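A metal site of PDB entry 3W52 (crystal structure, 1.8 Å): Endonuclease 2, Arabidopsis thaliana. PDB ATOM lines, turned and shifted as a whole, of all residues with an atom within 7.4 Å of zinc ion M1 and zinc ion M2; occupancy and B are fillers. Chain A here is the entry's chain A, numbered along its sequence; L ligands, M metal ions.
Zinc ion M2 is bound by an oxygen (O1) of LIG L1 (2.0 Å), a ring nitrogen (NE2) of His 6 (2.0 Å), the backbone nitrogen of Trp 1 (2.0 Å), the side-chain carboxylate of Asp 124 (2.1 Å) and the backbone carbonyl oxygen of Trp 1 (2.3 Å).
Zinc ion M2 has five donor atoms within binding distance.
Within 4 Å of zinc ion M1: Asp 45, His 58, His 120 and Asp 124.
Zinc ion M1 is bound by the side-chain carboxylate (OD2) of Asp 124 (2.1 Å), an oxygen (O1) of LIG L1 (2.1 Å), a ring nitrogen (NE2) of His 120 (2.1 Å), a ring nitrogen (ND1) of His 58 (2.2 Å), an oxygen (O2) of LIG L1 (2.5 Å) and the side-chain carboxylate (OD1) of Asp 45 (2.5 Å).
Zinc ion M1 has six donor atoms within binding distance.
A ring nitrogen (ND1) of His 120 is in hydrogen-bond range of the backbone carbonyl oxygen (O) of Cys 41 (2.8 Å).
ND1 of His 130 is in hydrogen-bond range of O of His 58, 2.8 Å away.
OD1 of Asp 45 sits close to NZ of Lys 48.
NE1 of Trp 1 is in hydrogen-bond range of O of Gly 123 (2.8 Å).
Of the 23 residues printed, 4 come within 4 Å of zinc ion M2.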
ATOM      1  N   TRP A   1      12.219  13.155 -11.879  1.00  0.00           N
ATOM      2  CA  TRP A   1      11.835  12.164 -12.927  1.00  0.00           C
ATOM      3  C   TRP A   1      10.324  12.080 -13.028  1.00  0.00           C
ATOM      4  O   TRP A   1       9.609  12.490 -12.112  1.00  0.00           O
ATOM      5  CB  TRP A   1      12.302  10.727 -12.497  1.00  0.00           C
ATOM      6  CG  TRP A   1      13.775  10.588 -12.139  1.00  0.00           C
ATOM      7  CD1 TRP A   1      14.348  10.607 -10.877  1.00  0.00           C
ATOM      8  CD2 TRP A   1      14.845  10.337 -13.075  1.00  0.00           C
ATOM      9  NE1 TRP A   1      15.723  10.349 -10.985  1.00  0.00           N
ATOM     10  CE2 TRP A   1      16.037  10.188 -12.297  1.00  0.00           C
ATOM     11  CE3 TRP A   1      14.909  10.221 -14.448  1.00  0.00           C
ATOM     12  CZ2 TRP A   1      17.285   9.940 -12.896  1.00  0.00           C
ATOM     13  CZ3 TRP A   1      16.166   9.973 -15.065  1.00  0.00           C
ATOM     14  CH2 TRP A   1      17.333   9.837 -14.276  1.00  0.00           C
ATOM     15  N   GLY A   2       9.888  11.494 -14.131  1.00  0.00           N
ATOM     16  CA  GLY A   2       8.479  11.180 -14.263  1.00  0.00           C
ATOM     17  C   GLY A   2       8.147   9.882 -13.544  1.00  0.00           C
ATOM     18  O   GLY A   2       8.932   9.304 -12.771  1.00  0.00           O
ATOM     19  N   LYS A   3       6.955   9.360 -13.819  1.00  0.00           N
ATOM     20  CA  LYS A   3       6.502   8.152 -13.089  1.00  0.00           C
ATOM     21  C   LYS A   3       7.400   6.927 -13.174  1.00  0.00           C
ATOM     22  O   LYS A   3       7.661   6.258 -12.162  1.00  0.00           O
ATOM     23  CB  LYS A   3       5.094   7.755 -13.597  1.00  0.00           C
ATOM     24  CG  LYS A   3       4.432   6.658 -12.777  1.00  0.00           C
ATOM     25  CD  LYS A   3       3.254   7.259 -11.923  1.00  0.00           C
ATOM     26  CE  LYS A   3       2.665   6.372 -10.780  1.00  0.00           C
ATOM     27  NZ  LYS A   3       3.534   6.252  -9.567  1.00  0.00           N
ATOM     28  N   GLY A   5      10.631   6.669 -13.860  1.00  0.00           N
ATOM     29  CA  GLY A   5      11.914   6.791 -13.136  1.00  0.00           C
ATOM     30  C   GLY A   5      11.726   6.599 -11.646  1.00  0.00           C
ATOM     31  O   GLY A   5      12.521   5.900 -10.981  1.00  0.00           O
ATOM     32  N   HIS A   6      10.715   7.235 -11.056  1.00  0.00           N
ATOM     33  CA  HIS A   6      10.528   7.057  -9.609  1.00  0.00           C
ATOM     34  C   HIS A   6      10.102   5.623  -9.289  1.00  0.00           C
ATOM     35  O   HIS A   6      10.498   5.057  -8.268  1.00  0.00           O
ATOM     36  CB  HIS A   6       9.439   8.024  -9.086  1.00  0.00           C
ATOM     37  CG  HIS A   6       9.940   9.428  -8.996  1.00  0.00           C
ATOM     38  ND1 HIS A   6      10.872   9.813  -8.049  1.00  0.00           N
ATOM     39  CD2 HIS A   6       9.767  10.477  -9.821  1.00  0.00           C
ATOM     40  CE1 HIS A   6      11.249  11.058  -8.294  1.00  0.00           C
ATOM     41  NE2 HIS A   6      10.585  11.481  -9.365  1.00  0.00           N
ATOM     42  N   CYS A  41       5.554   6.628  -5.007  1.00  0.00           N
ATOM     43  CA  CYS A  41       6.775   7.421  -5.214  1.00  0.00           C
ATOM     44  C   CYS A  41       6.582   8.697  -6.047  1.00  0.00           C
ATOM     45  O   CYS A  41       7.523   9.486  -6.164  1.00  0.00           O
ATOM     46  CB  CYS A  41       7.924   6.509  -5.720  1.00  0.00           C
ATOM     47  SG  CYS A  41       8.576   5.687  -4.172  1.00  0.00           S
ATOM     48  N   LEU A  42       5.371   8.928  -6.568  1.00  0.00           N
ATOM     49  CA  LEU A  42       5.058  10.184  -7.281  1.00  0.00           C
ATOM     50  C   LEU A  42       4.153  11.079  -6.418  1.00  0.00           C
ATOM     51  O   LEU A  42       3.794  12.193  -6.799  1.00  0.00           O
ATOM     52  CB  LEU A  42       4.403   9.947  -8.627  1.00  0.00           C
ATOM     53  CG  LEU A  42       4.806  10.796  -9.835  1.00  0.00           C
ATOM     54  CD1 LEU A  42       6.300  10.741 -10.162  1.00  0.00           C
ATOM     55  CD2 LEU A  42       4.041  10.216 -11.048  1.00  0.00           C
ATOM     56  N   ALA A  44       4.778  12.944  -3.980  1.00  0.00           N
ATOM     57  CA  ALA A  44       5.272  14.316  -3.806  1.00  0.00           C
ATOM     58  C   ALA A  44       4.933  15.218  -4.975  1.00  0.00           C
ATOM     59  O   ALA A  44       4.684  16.397  -4.796  1.00  0.00           O
ATOM     60  CB  ALA A  44       6.808  14.303  -3.583  1.00  0.00           C
ATOM     61  N   ASP A  45       4.946  14.690  -6.198  1.00  0.00           N
ATOM     62  CA  ASP A  45       4.620  15.575  -7.317  1.00  0.00           C
ATOM     63  C   ASP A  45       3.134  16.017  -7.259  1.00  0.00           C
ATOM     64  O   ASP A  45       2.795  17.089  -7.764  1.00  0.00           O
ATOM     65  CB  ASP A  45       4.870  14.856  -8.640  1.00  0.00           C
ATOM     66  CG  ASP A  45       6.304  14.978  -9.116  1.00  0.00           C
ATOM     67  OD1 ASP A  45       7.141  15.707  -8.509  1.00  0.00           O
ATOM     68  OD2 ASP A  45       6.600  14.344 -10.163  1.00  0.00           O
ATOM     69  N   LYS A  48       2.494  19.445  -5.105  1.00  0.00           N
ATOM     70  CA  LYS A  48       3.263  20.657  -5.444  1.00  0.00           C
ATOM     71  C   LYS A  48       2.366  21.941  -5.303  1.00  0.00           C
ATOM     72  O   LYS A  48       2.884  23.015  -5.042  1.00  0.00           O
ATOM     73  CB  LYS A  48       3.712  20.583  -6.913  1.00  0.00           C
ATOM     74  CG  LYS A  48       4.979  19.776  -7.109  1.00  0.00           C
ATOM     75  CD  LYS A  48       5.402  19.733  -8.589  1.00  0.00           C
ATOM     76  CE  LYS A  48       6.735  18.933  -8.644  1.00  0.00           C
ATOM     77  NZ  LYS A  48       7.064  18.650 -10.071  1.00  0.00           N
ATOM     78  N   SER A  55       7.170  23.021  -3.719  1.00  0.00           N
ATOM     79  CA  SER A  55       7.596  22.987  -5.110  1.00  0.00           C
ATOM     80  C   SER A  55       9.087  23.139  -5.371  1.00  0.00           C
ATOM     81  O   SER A  55       9.676  22.360  -6.138  1.00  0.00           O
ATOM     82  CB  SER A  55       6.798  24.021  -5.951  1.00  0.00           C
ATOM     83  OG  SER A  55       5.570  23.429  -6.354  1.00  0.00           O
ATOM     84  N   LEU A  57      11.409  22.291  -3.494  1.00  0.00           N
ATOM     85  CA  LEU A  57      12.134  21.205  -2.830  1.00  0.00           C
ATOM     86  C   LEU A  57      12.472  20.085  -3.806  1.00  0.00           C
ATOM     87  O   LEU A  57      13.132  19.138  -3.393  1.00  0.00           O
ATOM     88  CB  LEU A  57      11.315  20.620  -1.661  1.00  0.00           C
ATOM     89  CG  LEU A  57      10.960  21.678  -0.572  1.00  0.00           C
ATOM     90  CD1 LEU A  57      10.224  20.948   0.580  1.00  0.00           C
ATOM     91  CD2 LEU A  57      12.215  22.428  -0.078  1.00  0.00           C
ATOM     92  N   HIS A  58      11.985  20.150  -5.038  1.00  0.00           N
ATOM     93  CA  HIS A  58      12.281  19.068  -6.000  1.00  0.00           C
ATOM     94  C   HIS A  58      13.556  19.250  -6.772  1.00  0.00           C
ATOM     95  O   HIS A  58      13.990  18.287  -7.458  1.00  0.00           O
ATOM     96  CB  HIS A  58      11.152  18.940  -7.039  1.00  0.00           C
ATOM     97  CG  HIS A  58       9.851  18.515  -6.436  1.00  0.00           C
ATOM     98  ND1 HIS A  58       9.266  17.295  -6.741  1.00  0.00           N
ATOM     99  CD2 HIS A  58       9.069  19.088  -5.506  1.00  0.00           C
ATOM    100  CE1 HIS A  58       8.171  17.146  -6.018  1.00  0.00           C
ATOM    101  NE2 HIS A  58       8.022  18.221  -5.252  1.00  0.00           N
ATOM    102  N   TYR A  59      14.195  20.425  -6.685  1.00  0.00           N
ATOM    103  CA  TYR A  59      15.385  20.594  -7.528  1.00  0.00           C
ATOM    104  C   TYR A  59      16.372  21.592  -6.861  1.00  0.00           C
ATOM    105  O   TYR A  59      16.131  22.010  -5.734  1.00  0.00           O
ATOM    106  CB  TYR A  59      14.996  21.144  -8.889  1.00  0.00           C
ATOM    107  CG  TYR A  59      14.145  22.403  -8.760  1.00  0.00           C
ATOM    108  CD1 TYR A  59      14.744  23.658  -8.581  1.00  0.00           C
ATOM    109  CD2 TYR A  59      12.743  22.323  -8.777  1.00  0.00           C
ATOM    110  CE1 TYR A  59      13.986  24.821  -8.420  1.00  0.00           C
ATOM    111  CE2 TYR A  59      11.976  23.495  -8.609  1.00  0.00           C
ATOM    112  CZ  TYR A  59      12.621  24.716  -8.431  1.00  0.00           C
ATOM    113  OH  TYR A  59      11.830  25.869  -8.296  1.00  0.00           O
ATOM    114  N   HIS A 120      10.724  10.185  -2.859  1.00  0.00           N
ATOM    115  CA  HIS A 120      10.689  10.957  -4.107  1.00  0.00           C
ATOM    116  C   HIS A 120      11.954  11.868  -4.292  1.00  0.00           C
ATOM    117  O   HIS A 120      12.540  11.913  -5.376  1.00  0.00           O
ATOM    118  CB  HIS A 120       9.423  11.839  -4.087  1.00  0.00           C
ATOM    119  CG  HIS A 120       9.214  12.588  -5.362  1.00  0.00           C
ATOM    120  ND1 HIS A 120       8.476  12.060  -6.406  1.00  0.00           N
ATOM    121  CD2 HIS A 120       9.648  13.802  -5.768  1.00  0.00           C
ATOM    122  CE1 HIS A 120       8.475  12.925  -7.417  1.00  0.00           C
ATOM    123  NE2 HIS A 120       9.179  13.988  -7.058  1.00  0.00           N
ATOM    124  N   PHE A 121      12.330  12.603  -3.250  1.00  0.00           N
ATOM    125  CA  PHE A 121      13.467  13.515  -3.351  1.00  0.00           C
ATOM    126  C   PHE A 121      14.804  12.808  -3.558  1.00  0.00           C
ATOM    127  O   PHE A 121      15.631  13.303  -4.283  1.00  0.00           O
ATOM    128  CB  PHE A 121      13.521  14.511  -2.171  1.00  0.00           C
ATOM    129  CG  PHE A 121      12.327  15.427  -2.106  1.00  0.00           C
ATOM    130  CD1 PHE A 121      11.759  15.937  -3.252  1.00  0.00           C
ATOM    131  CD2 PHE A 121      11.776  15.773  -0.871  1.00  0.00           C
ATOM    132  CE1 PHE A 121      10.623  16.833  -3.203  1.00  0.00           C
ATOM    133  CE2 PHE A 121      10.672  16.656  -0.796  1.00  0.00           C
ATOM    134  CZ  PHE A 121      10.108  17.180  -1.940  1.00  0.00           C
ATOM    135  N   GLY A 123      15.057  10.310  -5.323  1.00  0.00           N
ATOM    136  CA  GLY A 123      15.024  10.070  -6.732  1.00  0.00           C
ATOM    137  C   GLY A 123      15.352  11.354  -7.508  1.00  0.00           C
ATOM    138  O   GLY A 123      16.213  11.356  -8.374  1.00  0.00           O
ATOM    139  N   ASP A 124      14.663  12.458  -7.205  1.00  0.00           N
ATOM    140  CA  ASP A 124      14.866  13.684  -7.962  1.00  0.00           C
ATOM    141  C   ASP A 124      16.299  14.208  -7.906  1.00  0.00           C
ATOM    142  O   ASP A 124      16.781  14.761  -8.880  1.00  0.00           O
ATOM    143  CB  ASP A 124      13.881  14.753  -7.467  1.00  0.00           C
ATOM    144  CG  ASP A 124      12.538  14.697  -8.174  1.00  0.00           C
ATOM    145  OD1 ASP A 124      12.381  13.826  -9.027  1.00  0.00           O
ATOM    146  OD2 ASP A 124      11.682  15.545  -7.885  1.00  0.00           O
ATOM    147  N   ILE A 125      16.962  14.054  -6.746  1.00  0.00           N
ATOM    148  CA  ILE A 125      18.320  14.594  -6.658  1.00  0.00           C
ATOM    149  C   ILE A 125      19.296  13.826  -7.565  1.00  0.00           C
ATOM    150  O   ILE A 125      20.421  14.257  -7.753  1.00  0.00           O
ATOM    151  CB  ILE A 125      18.828  14.657  -5.205  1.00  0.00           C
ATOM    152  CG1 ILE A 125      20.017  15.626  -5.116  1.00  0.00           C
ATOM    153  CG2 ILE A 125      19.291  13.288  -4.722  1.00  0.00           C
ATOM    154  CD1 ILE A 125      20.314  15.978  -3.583  1.00  0.00           C
ATOM    155  N   GLN A 127      18.332  12.996 -10.783  1.00  0.00           N
ATOM    156  CA  GLN A 127      18.023  13.369 -12.195  1.00  0.00           C
ATOM    157  C   GLN A 127      18.988  14.534 -12.464  1.00  0.00           C
ATOM    158  O   GLN A 127      18.894  15.579 -11.805  1.00  0.00           O
ATOM    159  CB  GLN A 127      16.511  13.814 -12.271  1.00  0.00           C
ATOM    160  CG  GLN A 127      15.864  13.595 -13.658  1.00  0.00           C
ATOM    161  CD  GLN A 127      16.279  14.620 -14.715  1.00  0.00           C
ATOM    162  OE1 GLN A 127      17.424  14.751 -15.017  1.00  0.00           O
ATOM    163  NE2 GLN A 127      15.307  15.332 -15.287  1.00  0.00           N
ATOM    164  N   HIS A 130      17.740  18.003 -12.506  1.00  0.00           N
ATOM    165  CA  HIS A 130      17.181  18.590 -11.295  1.00  0.00           C
ATOM    166  C   HIS A 130      18.280  19.293 -10.466  1.00  0.00           C
ATOM    167  O   HIS A 130      17.992  19.802  -9.383  1.00  0.00           O
ATOM    168  CB  HIS A 130      16.487  17.559 -10.412  1.00  0.00           C
ATOM    169  CG  HIS A 130      15.091  17.279 -10.881  1.00  0.00           C
ATOM    170  ND1 HIS A 130      13.987  17.363 -10.061  1.00  0.00           N
ATOM    171  CD2 HIS A 130      14.632  16.982 -12.114  1.00  0.00           C
ATOM    172  CE1 HIS A 130      12.891  17.144 -10.764  1.00  0.00           C
ATOM    173  NE2 HIS A 130      13.260  16.909 -12.017  1.00  0.00           N
ATOM    174  N   HIS A 154      14.369  19.134 -20.317  1.00  0.00           N
ATOM    175  CA  HIS A 154      14.091  18.639 -18.970  1.00  0.00           C
ATOM    176  C   HIS A 154      13.180  17.402 -19.042  1.00  0.00           C
ATOM    177  O   HIS A 154      13.458  16.386 -18.399  1.00  0.00           O
ATOM    178  CB  HIS A 154      13.439  19.677 -18.077  1.00  0.00           C
ATOM    179  CG  HIS A 154      13.325  19.237 -16.642  1.00  0.00           C
ATOM    180  ND1 HIS A 154      14.266  19.543 -15.669  1.00  0.00           N
ATOM    181  CD2 HIS A 154      12.421  18.426 -16.044  1.00  0.00           C
ATOM    182  CE1 HIS A 154      13.926  18.946 -14.540  1.00  0.00           C
ATOM    183  NE2 HIS A 154      12.816  18.252 -14.745  1.00  0.00           N
ATOM    184  N   ASP A 158      13.426  13.595 -17.649  1.00  0.00           N
ATOM    185  CA  ASP A 158      12.506  13.042 -16.626  1.00  0.00           C
ATOM    186  C   ASP A 158      11.774  11.815 -17.198  1.00  0.00           C
ATOM    187  O   ASP A 158      11.510  10.868 -16.478  1.00  0.00           O
ATOM    188  CB  ASP A 158      11.347  14.023 -16.345  1.00  0.00           C
ATOM    189  CG  ASP A 158      11.647  15.035 -15.226  1.00  0.00           C
ATOM    190  OD1 ASP A 158      12.631  14.888 -14.490  1.00  0.00           O
ATOM    191  OD2 ASP A 158      10.822  15.994 -15.120  1.00  0.00           O
HETATM  192  S1  LIG L   1       9.470  15.952 -11.061  1.00  0.00           S
HETATM  193  O1  LIG L   1       9.689  14.808 -10.104  1.00  0.00           O
HETATM  194  O2  LIG L   1       9.553  17.223 -10.184  1.00  0.00           O
HETATM  195  O3  LIG L   1      10.410  15.906 -12.167  1.00  0.00           O
HETATM  196  O4  LIG L   1       8.039  15.756 -11.589  1.00  0.00           O
HETATM  197  N1  LG2 L   2      11.698  21.103 -12.444  1.00  0.00           N
HETATM  198  C1  LG2 L   2      10.642  22.001 -12.358  1.00  0.00           C
HETATM  199  N2  LG2 L   2      11.035  23.258 -12.276  1.00  0.00           N
HETATM  200  C2  LG2 L   2      12.422  23.185 -12.300  1.00  0.00           C
HETATM  201  C3  LG2 L   2      13.403  24.169 -12.243  1.00  0.00           C
HETATM  202  N3  LG2 L   2      13.116  25.467 -12.158  1.00  0.00           N
HETATM  203  N4  LG2 L   2      14.695  23.784 -12.281  1.00  0.00           N
HETATM  204  C4  LG2 L   2      14.971  22.445 -12.370  1.00  0.00           C
HETATM  205  N5  LG2 L   2      14.126  21.425 -12.431  1.00  0.00           N
HETATM  206  C5  LG2 L   2      12.849  21.864 -12.385  1.00  0.00           C
HETATM  207 ZN    ZN M   1       9.622  15.733  -8.208  1.00  0.00          ZN
HETATM  208 ZN    ZN M   2      10.875  13.210 -10.355  1.00  0.00          ZN
HETATM  209 ZN    ZN M   3      11.673  16.991 -13.445  1.00  0.00          ZN
